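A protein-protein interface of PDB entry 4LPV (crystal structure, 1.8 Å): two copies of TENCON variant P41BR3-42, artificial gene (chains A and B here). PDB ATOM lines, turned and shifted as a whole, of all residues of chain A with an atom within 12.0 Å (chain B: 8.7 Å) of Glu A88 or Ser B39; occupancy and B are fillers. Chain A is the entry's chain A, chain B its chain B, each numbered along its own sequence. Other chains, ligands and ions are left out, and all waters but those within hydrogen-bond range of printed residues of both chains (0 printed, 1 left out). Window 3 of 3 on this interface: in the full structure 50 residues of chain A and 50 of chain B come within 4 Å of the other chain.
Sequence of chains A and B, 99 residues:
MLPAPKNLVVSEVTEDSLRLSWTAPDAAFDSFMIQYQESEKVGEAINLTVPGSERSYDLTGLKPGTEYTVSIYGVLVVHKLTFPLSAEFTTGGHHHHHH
The backbone NH (N) of Thr A91 sits at hydrogen-bond distance from the backbone carbonyl oxygen (O) of Thr B66, at 2.9 Å.
OG of Ser A86 is in hydrogen-bond range of OG of Ser B71 (3.0 Å).
The backbone NH of Val B70 lies within hydrogen-bond range of the backbone carbonyl oxygen of Ala A87.
N of Tyr B68 sits at hydrogen-bond distance from O of Phe A89 (2.7 Å).
The side-chain carboxylate (OE2) of Glu A88 lies within hydrogen-bond range of the side-chain hydroxyl (OG1) of Thr B69, at 3.2 Å.
The backbone NH (N) of Ser B39 lies within hydrogen-bond range of the backbone carbonyl oxygen (O) of Glu B67 (2.8 Å).
OG of Ser B39 lies within hydrogen-bond range of OG1 of Thr B69.
The backbone carbonyl oxygen (O) of Gln B37 lies within hydrogen-bond range of the backbone NH (N) of Thr B69 (2.8 Å).
Leu A85 touches Ser B71 (O to CA, 3.3 Å).
Ser A86 touches Val B70.
Leu B8 touches Ala A87 (CD2 to CB, 3.9 Å).
Ala A87 touches Thr B69.
Glu A88 touches Tyr B68.
O of Thr B66 touches O of Phe A89, 3.7 Å away.
Leu B18 touches Thr A90.
Thr B66 touches Thr A90 (O to CA, 3.3 Å).
Val B13 touches Thr A91.
Tyr B68 touches Thr A91.
Pro A84 touches none of the printed residues of chain B.
Printed residues of chain B within 4 Å of Ser A86: Val B70 and Ser B71.
Ala A87 touches just these residues of chain B: Leu B8 (3.9 Å), Tyr B68 (3.7 Å), Thr B69 (3.4 Å) and Val B70 (2.7 Å).
Of chain B, only Ser B39 (3.5 Å), Glu B67 (3.7 Å), Tyr B68 (3.2 Å) and Thr B69 (3.2 Å) come within 4 Å of Glu A88.
Phe A89 touches just these residues of chain B: Leu B8, Val B9, Val B10, Leu B18, Thr B66, Glu B67 and Tyr B68.
Of the printed residues of chain B, Thr A90 touches Val B13 (3.5 Å), Leu B18 (3.9 Å), Thr B66 (3.3 Å) and Glu B67 (3.7 Å).
Leu B20 touches none of the printed residues of chain A.
No residue of chain A comes within 4 Å of Gln B37.
Ser B39 touches just one residue of chain A: Glu A88.
No residue of chain A comes within 4 Å of Glu B40.
No residue of chain A comes within 4 Å of Lys B41.
Printed residues of chain A within 4 Å of Thr B66: Phe A89, Thr A90 and Thr A91.
Glu B67 touches just these residues of chain A: Glu A88, Phe A89 and Thr A90.
Tyr B68 touches just these residues of chain A: Ala A87 (3.7 Å), Glu A88 (3.2 Å), Phe A89 (2.7 Å) and Thr A91 (3.9 Å).
Of chain A, only Leu A85 (3.6 Å), Ser A86 (3.2 Å) and Ala A87 (2.7 Å) come within 4 Å of Val B70.
Of the printed residues of chain A, Ser B71 touches Leu A85 (3.3 Å) and Ser A86 (3.0 Å).
The nearest residue of chain B that does not touch Glu A88 is Val B70 (4.8 Å).
Of the 19 printed residues of chain B, 12 touch a printed residue of chain A.
Hydrophobic or aromatic side chains of chain B that line the printed part of chain A: Leu B8, Val B10, Val B13, Leu B18, Tyr B68 and Val B70.
Of the 10 printed residues of chain A, 8 touch a printed residue of chain B.
Hydrophobic or aromatic side chains of chain A within 4 Å of the printed part of chain B: Leu A85, Ala A87 and Phe A89.
Among the printed residues, 28 pairs touch across the chains.
No position is printed for both chains.
Of the 28 pairs that touch across the chains among the printed residues, none has its exchanged pair printed and touching as well.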
ATOM      1  N   PRO A  84     -22.825  29.602  18.551  1.00  0.00           N
ATOM      2  CA  PRO A  84     -21.959  28.481  18.945  1.00  0.00           C
ATOM      3  C   PRO A  84     -22.563  27.094  18.649  1.00  0.00           C
ATOM      4  O   PRO A  84     -23.785  26.947  18.534  1.00  0.00           O
ATOM      5  CB  PRO A  84     -21.785  28.693  20.458  1.00  0.00           C
ATOM      6  CG  PRO A  84     -23.010  29.427  20.873  1.00  0.00           C
ATOM      7  CD  PRO A  84     -23.393  30.306  19.715  1.00  0.00           C
ATOM      8  N   LEU A  85     -21.695  26.100  18.470  1.00  0.00           N
ATOM      9  CA  LEU A  85     -22.093  24.702  18.582  1.00  0.00           C
ATOM     10  C   LEU A  85     -21.442  24.156  19.846  1.00  0.00           C
ATOM     11  O   LEU A  85     -20.218  24.149  19.970  1.00  0.00           O
ATOM     12  CB  LEU A  85     -21.660  23.874  17.371  1.00  0.00           C
ATOM     13  CG  LEU A  85     -22.024  22.379  17.463  1.00  0.00           C
ATOM     14  CD1 LEU A  85     -23.529  22.189  17.571  1.00  0.00           C
ATOM     15  CD2 LEU A  85     -21.489  21.591  16.303  1.00  0.00           C
ATOM     16  N   SER A  86     -22.269  23.717  20.789  1.00  0.00           N
ATOM     17  CA  SER A  86     -21.781  23.263  22.083  1.00  0.00           C
ATOM     18  C   SER A  86     -21.968  21.762  22.260  1.00  0.00           C
ATOM     19  O   SER A  86     -22.956  21.190  21.796  1.00  0.00           O
ATOM     20  CB  SER A  86     -22.502  23.999  23.213  1.00  0.00           C
ATOM     21  OG  SER A  86     -22.395  25.404  23.065  1.00  0.00           O
ATOM     22  N   ALA A  87     -21.009  21.137  22.939  1.00  0.00           N
ATOM     23  CA  ALA A  87     -21.097  19.723  23.284  1.00  0.00           C
ATOM     24  C   ALA A  87     -20.391  19.474  24.611  1.00  0.00           C
ATOM     25  O   ALA A  87     -19.547  20.265  25.030  1.00  0.00           O
ATOM     26  CB  ALA A  87     -20.490  18.859  22.191  1.00  0.00           C
ATOM     27  N   GLU A  88     -20.749  18.384  25.283  1.00  0.00           N
ATOM     28  CA  GLU A  88     -20.026  17.977  26.481  1.00  0.00           C
ATOM     29  C   GLU A  88     -19.233  16.702  26.222  1.00  0.00           C
ATOM     30  O   GLU A  88     -19.736  15.758  25.600  1.00  0.00           O
ATOM     31  CB  GLU A  88     -20.971  17.783  27.671  1.00  0.00           C
ATOM     32  CG  GLU A  88     -21.346  19.060  28.391  1.00  0.00           C
ATOM     33  CD  GLU A  88     -22.623  19.665  27.859  1.00  0.00           C
ATOM     34  OE1 GLU A  88     -23.577  18.899  27.618  1.00  0.00           O
ATOM     35  OE2 GLU A  88     -22.673  20.899  27.669  1.00  0.00           O
ATOM     36  N   PHE A  89     -17.988  16.691  26.691  1.00  0.00           N
ATOM     37  CA  PHE A  89     -17.140  15.505  26.615  1.00  0.00           C
ATOM     38  C   PHE A  89     -16.471  15.269  27.962  1.00  0.00           C
ATOM     39  O   PHE A  89     -16.125  16.221  28.668  1.00  0.00           O
ATOM     40  CB  PHE A  89     -16.067  15.647  25.526  1.00  0.00           C
ATOM     41  CG  PHE A  89     -16.612  16.026  24.185  1.00  0.00           C
ATOM     42  CD1 PHE A  89     -17.296  15.102  23.412  1.00  0.00           C
ATOM     43  CD2 PHE A  89     -16.435  17.314  23.692  1.00  0.00           C
ATOM     44  CE1 PHE A  89     -17.804  15.451  22.173  1.00  0.00           C
ATOM     45  CE2 PHE A  89     -16.938  17.672  22.454  1.00  0.00           C
ATOM     46  CZ  PHE A  89     -17.623  16.740  21.689  1.00  0.00           C
ATOM     47  N   THR A  90     -16.294  13.998  28.313  1.00  0.00           N
ATOM     48  CA  THR A  90     -15.594  13.637  29.540  1.00  0.00           C
ATOM     49  C   THR A  90     -14.220  13.061  29.199  1.00  0.00           C
ATOM     50  O   THR A  90     -14.093  12.202  28.326  1.00  0.00           O
ATOM     51  CB  THR A  90     -16.430  12.650  30.405  1.00  0.00           C
ATOM     52  OG1 THR A  90     -17.736  13.190  30.622  1.00  0.00           O
ATOM     53  CG2 THR A  90     -15.776  12.407  31.754  1.00  0.00           C
ATOM     54  N   THR A  91     -13.185  13.564  29.861  1.00  0.00           N
ATOM     55  CA  THR A  91     -11.846  13.019  29.686  1.00  0.00           C
ATOM     56  C   THR A  91     -11.829  11.607  30.266  1.00  0.00           C
ATOM     57  O   THR A  91     -12.733  11.223  31.009  1.00  0.00           O
ATOM     58  CB  THR A  91     -10.762  13.889  30.378  1.00  0.00           C
ATOM     59  OG1 THR A  91     -11.152  14.150  31.730  1.00  0.00           O
ATOM     60  CG2 THR A  91     -10.587  15.229  29.656  1.00  0.00           C
ATOM     61  N   GLY A  92     -10.806  10.838  29.915  1.00  0.00           N
ATOM     62  CA  GLY A  92     -10.648   9.502  30.455  1.00  0.00           C
ATOM     63  C   GLY A  92     -10.075   9.498  31.863  1.00  0.00           C
ATOM     64  O   GLY A  92      -9.584  10.528  32.344  1.00  0.00           O
ATOM     65  N   HIS A  95     -12.311  10.529  38.410  1.00  0.00           N
ATOM     66  CA  HIS A  95     -12.671  11.930  38.714  1.00  0.00           C
ATOM     67  C   HIS A  95     -12.280  12.521  40.078  1.00  0.00           C
ATOM     68  O   HIS A  95     -13.116  13.165  40.726  1.00  0.00           O
ATOM     69  CB  HIS A  95     -14.168  12.108  38.530  1.00  0.00           C
ATOM     70  N   LEU B   8     -19.878  18.551  16.125  1.00  0.00           N
ATOM     71  CA  LEU B   8     -18.806  18.564  17.123  1.00  0.00           C
ATOM     72  C   LEU B   8     -18.781  17.250  17.922  1.00  0.00           C
ATOM     73  O   LEU B   8     -19.713  16.928  18.651  1.00  0.00           O
ATOM     74  CB  LEU B   8     -18.902  19.790  18.050  1.00  0.00           C
ATOM     75  CG  LEU B   8     -17.819  19.942  19.138  1.00  0.00           C
ATOM     76  CD1 LEU B   8     -16.420  20.027  18.535  1.00  0.00           C
ATOM     77  CD2 LEU B   8     -18.085  21.133  20.057  1.00  0.00           C
ATOM     78  N   VAL B   9     -17.711  16.486  17.732  1.00  0.00           N
ATOM     79  CA  VAL B   9     -17.501  15.217  18.413  1.00  0.00           C
ATOM     80  C   VAL B   9     -16.038  15.185  18.869  1.00  0.00           C
ATOM     81  O   VAL B   9     -15.287  16.140  18.634  1.00  0.00           O
ATOM     82  CB  VAL B   9     -17.808  13.983  17.491  1.00  0.00           C
ATOM     83  CG1 VAL B   9     -19.250  13.996  16.986  1.00  0.00           C
ATOM     84  CG2 VAL B   9     -16.824  13.893  16.316  1.00  0.00           C
ATOM     85  N   VAL B  10     -15.644  14.109  19.544  1.00  0.00           N
ATOM     86  CA  VAL B  10     -14.226  13.809  19.722  1.00  0.00           C
ATOM     87  C   VAL B  10     -13.844  12.615  18.843  1.00  0.00           C
ATOM     88  O   VAL B  10     -14.666  11.735  18.595  1.00  0.00           O
ATOM     89  CB  VAL B  10     -13.847  13.550  21.211  1.00  0.00           C
ATOM     90  CG1 VAL B  10     -13.847  14.858  22.003  1.00  0.00           C
ATOM     91  CG2 VAL B  10     -14.774  12.522  21.843  1.00  0.00           C
ATOM     92  N   VAL B  13      -9.999  10.514  22.962  1.00  0.00           N
ATOM     93  CA  VAL B  13     -10.009  10.986  24.341  1.00  0.00           C
ATOM     94  C   VAL B  13      -8.866  10.306  25.096  1.00  0.00           C
ATOM     95  O   VAL B  13      -8.624   9.110  24.916  1.00  0.00           O
ATOM     96  CB  VAL B  13     -11.355  10.678  25.040  1.00  0.00           C
ATOM     97  CG1 VAL B  13     -11.338  11.148  26.482  1.00  0.00           C
ATOM     98  CG2 VAL B  13     -12.507  11.326  24.291  1.00  0.00           C
ATOM     99  N   LEU B  18      -8.806  15.967  24.951  1.00  0.00           N
ATOM    100  CA  LEU B  18      -9.960  15.718  24.097  1.00  0.00           C
ATOM    101  C   LEU B  18      -9.592  16.158  22.677  1.00  0.00           C
ATOM    102  O   LEU B  18      -9.316  17.331  22.449  1.00  0.00           O
ATOM    103  CB  LEU B  18     -11.163  16.533  24.584  1.00  0.00           C
ATOM    104  CG  LEU B  18     -11.768  16.253  25.962  1.00  0.00           C
ATOM    105  CD1 LEU B  18     -12.759  17.350  26.351  1.00  0.00           C
ATOM    106  CD2 LEU B  18     -12.444  14.886  25.970  1.00  0.00           C
ATOM    107  N   LEU B  20     -10.869  17.182  19.443  1.00  0.00           N
ATOM    108  CA  LEU B  20     -12.097  17.660  18.821  1.00  0.00           C
ATOM    109  C   LEU B  20     -12.081  17.446  17.308  1.00  0.00           C
ATOM    110  O   LEU B  20     -11.020  17.476  16.675  1.00  0.00           O
ATOM    111  CB  LEU B  20     -12.304  19.148  19.133  1.00  0.00           C
ATOM    112  CG  LEU B  20     -12.122  19.592  20.587  1.00  0.00           C
ATOM    113  CD1 LEU B  20     -12.144  21.109  20.709  1.00  0.00           C
ATOM    114  CD2 LEU B  20     -13.190  18.954  21.484  1.00  0.00           C
ATOM    115  N   TYR B  36     -13.716  26.316  26.103  1.00  0.00           N
ATOM    116  CA  TYR B  36     -13.960  25.138  26.941  1.00  0.00           C
ATOM    117  C   TYR B  36     -13.889  25.452  28.440  1.00  0.00           C
ATOM    118  O   TYR B  36     -13.108  26.303  28.894  1.00  0.00           O
ATOM    119  CB  TYR B  36     -13.012  23.989  26.572  1.00  0.00           C
ATOM    120  CG  TYR B  36     -11.544  24.267  26.871  1.00  0.00           C
ATOM    121  CD1 TYR B  36     -10.810  25.142  26.086  1.00  0.00           C
ATOM    122  CD2 TYR B  36     -10.906  23.653  27.940  1.00  0.00           C
ATOM    123  CE1 TYR B  36      -9.501  25.398  26.340  1.00  0.00           C
ATOM    124  CE2 TYR B  36      -9.559  23.888  28.224  1.00  0.00           C
ATOM    125  CZ  TYR B  36      -8.862  24.771  27.408  1.00  0.00           C
ATOM    126  OH  TYR B  36      -7.541  25.056  27.639  1.00  0.00           O
ATOM    127  N   GLN B  37     -14.751  24.779  29.196  1.00  0.00           N
ATOM    128  CA  GLN B  37     -14.848  24.977  30.634  1.00  0.00           C
ATOM    129  C   GLN B  37     -15.341  23.671  31.274  1.00  0.00           C
ATOM    130  O   GLN B  37     -16.140  22.943  30.678  1.00  0.00           O
ATOM    131  CB  GLN B  37     -15.806  26.143  30.946  1.00  0.00           C
ATOM    132  CG  GLN B  37     -15.881  26.542  32.418  1.00  0.00           C
ATOM    133  CD  GLN B  37     -16.656  27.841  32.656  1.00  0.00           C
ATOM    134  OE1 GLN B  37     -17.459  28.264  31.830  1.00  0.00           O
ATOM    135  NE2 GLN B  37     -16.408  28.473  33.797  1.00  0.00           N
ATOM    136  N   GLU B  38     -14.849  23.365  32.473  1.00  0.00           N
ATOM    137  CA  GLU B  38     -15.424  22.283  33.275  1.00  0.00           C
ATOM    138  C   GLU B  38     -16.927  22.504  33.469  1.00  0.00           C
ATOM    139  O   GLU B  38     -17.356  23.596  33.859  1.00  0.00           O
ATOM    140  CB  GLU B  38     -14.754  22.204  34.647  1.00  0.00           C
ATOM    141  CG  GLU B  38     -13.289  21.816  34.646  1.00  0.00           C
ATOM    142  CD  GLU B  38     -12.763  21.618  36.055  1.00  0.00           C
ATOM    143  OE1 GLU B  38     -13.545  21.166  36.920  1.00  0.00           O
ATOM    144  OE2 GLU B  38     -11.578  21.930  36.304  1.00  0.00           O
ATOM    145  N   SER B  39     -17.722  21.467  33.211  1.00  0.00           N
ATOM    146  CA  SER B  39     -19.177  21.547  33.355  1.00  0.00           C
ATOM    147  C   SER B  39     -19.657  21.860  34.784  1.00  0.00           C
ATOM    148  O   SER B  39     -20.851  22.079  35.007  1.00  0.00           O
ATOM    149  CB  SER B  39     -19.845  20.266  32.848  1.00  0.00           C
ATOM    150  OG  SER B  39     -20.106  20.336  31.455  1.00  0.00           O
ATOM    151  N   GLU B  40     -18.731  21.869  35.745  1.00  0.00           N
ATOM    152  CA  GLU B  40     -19.036  22.288  37.113  1.00  0.00           C
ATOM    153  C   GLU B  40     -18.847  23.792  37.258  1.00  0.00           C
ATOM    154  O   GLU B  40     -19.559  24.580  36.630  1.00  0.00           O
ATOM    155  CB  GLU B  40     -18.162  21.547  38.115  1.00  0.00           C
ATOM    156  N   LYS B  41     -17.883  24.192  38.081  1.00  0.00           N
ATOM    157  CA  LYS B  41     -17.644  25.611  38.324  1.00  0.00           C
ATOM    158  C   LYS B  41     -16.245  25.860  38.871  1.00  0.00           C
ATOM    159  O   LYS B  41     -16.080  26.417  39.960  1.00  0.00           O
ATOM    160  CB  LYS B  41     -18.700  26.180  39.274  1.00  0.00           C
ATOM    161  N   VAL B  42     -15.240  25.438  38.112  1.00  0.00           N
ATOM    162  CA  VAL B  42     -13.850  25.682  38.485  1.00  0.00           C
ATOM    163  C   VAL B  42     -13.285  26.910  37.760  1.00  0.00           C
ATOM    164  O   VAL B  42     -12.181  26.866  37.213  1.00  0.00           O
ATOM    165  CB  VAL B  42     -12.994  24.443  38.221  1.00  0.00           C
ATOM    166  N   THR B  66     -13.117  14.197  33.921  1.00  0.00           N
ATOM    167  CA  THR B  66     -13.798  15.485  34.074  1.00  0.00           C
ATOM    168  C   THR B  66     -14.621  15.805  32.826  1.00  0.00           C
ATOM    169  O   THR B  66     -14.136  15.650  31.702  1.00  0.00           O
ATOM    170  CB  THR B  66     -12.766  16.621  34.353  1.00  0.00           C
ATOM    171  OG1 THR B  66     -12.028  16.322  35.546  1.00  0.00           O
ATOM    172  CG2 THR B  66     -13.447  17.964  34.530  1.00  0.00           C
ATOM    173  N   GLU B  67     -15.872  16.222  33.027  1.00  0.00           N
ATOM    174  CA  GLU B  67     -16.709  16.676  31.923  1.00  0.00           C
ATOM    175  C   GLU B  67     -16.427  18.139  31.569  1.00  0.00           C
ATOM    176  O   GLU B  67     -16.471  19.028  32.433  1.00  0.00           O
ATOM    177  CB  GLU B  67     -18.204  16.489  32.214  1.00  0.00           C
ATOM    178  CG  GLU B  67     -19.093  16.967  31.056  1.00  0.00           C
ATOM    179  CD  GLU B  67     -20.574  16.642  31.219  1.00  0.00           C
ATOM    180  OE1 GLU B  67     -21.312  17.456  31.823  1.00  0.00           O
ATOM    181  OE2 GLU B  67     -21.006  15.580  30.716  1.00  0.00           O
ATOM    182  N   TYR B  68     -16.136  18.371  30.291  1.00  0.00           N
ATOM    183  CA  TYR B  68     -15.951  19.722  29.764  1.00  0.00           C
ATOM    184  C   TYR B  68     -17.077  20.080  28.793  1.00  0.00           C
ATOM    185  O   TYR B  68     -17.505  19.246  27.995  1.00  0.00           O
ATOM    186  CB  TYR B  68     -14.583  19.846  29.075  1.00  0.00           C
ATOM    187  CG  TYR B  68     -13.419  19.799  30.041  1.00  0.00           C
ATOM    188  CD1 TYR B  68     -12.891  18.579  30.478  1.00  0.00           C
ATOM    189  CD2 TYR B  68     -12.851  20.973  30.530  1.00  0.00           C
ATOM    190  CE1 TYR B  68     -11.828  18.535  31.371  1.00  0.00           C
ATOM    191  CE2 TYR B  68     -11.794  20.940  31.419  1.00  0.00           C
ATOM    192  CZ  TYR B  68     -11.292  19.721  31.843  1.00  0.00           C
ATOM    193  OH  TYR B  68     -10.239  19.700  32.725  1.00  0.00           O
ATOM    194  N   THR B  69     -17.574  21.312  28.891  1.00  0.00           N
ATOM    195  CA  THR B  69     -18.478  21.855  27.888  1.00  0.00           C
ATOM    196  C   THR B  69     -17.602  22.558  26.874  1.00  0.00           C
ATOM    197  O   THR B  69     -16.790  23.414  27.239  1.00  0.00           O
ATOM    198  CB  THR B  69     -19.474  22.870  28.479  1.00  0.00           C
ATOM    199  OG1 THR B  69     -20.368  22.201  29.377  1.00  0.00           O
ATOM    200  CG2 THR B  69     -20.280  23.522  27.370  1.00  0.00           C
ATOM    201  N   VAL B  70     -17.736  22.166  25.612  1.00  0.00           N
ATOM    202  CA  VAL B  70     -16.927  22.729  24.540  1.00  0.00           C
ATOM    203  C   VAL B  70     -17.818  23.451  23.552  1.00  0.00           C
ATOM    204  O   VAL B  70     -18.754  22.863  23.020  1.00  0.00           O
ATOM    205  CB  VAL B  70     -16.130  21.635  23.792  1.00  0.00           C
ATOM    206  CG1 VAL B  70     -15.472  22.222  22.550  1.00  0.00           C
ATOM    207  CG2 VAL B  70     -15.091  21.001  24.714  1.00  0.00           C
ATOM    208  N   SER B  71     -17.535  24.733  23.320  1.00  0.00           N
ATOM    209  CA  SER B  71     -18.245  25.514  22.307  1.00  0.00           C
ATOM    210  C   SER B  71     -17.316  25.873  21.144  1.00  0.00           C
ATOM    211  O   SER B  71     -16.194  26.328  21.358  1.00  0.00           O
ATOM    212  CB  SER B  71     -18.842  26.789  22.914  1.00  0.00           C
ATOM    213  OG  SER B  71     -19.710  26.497  23.999  1.00  0.00           O
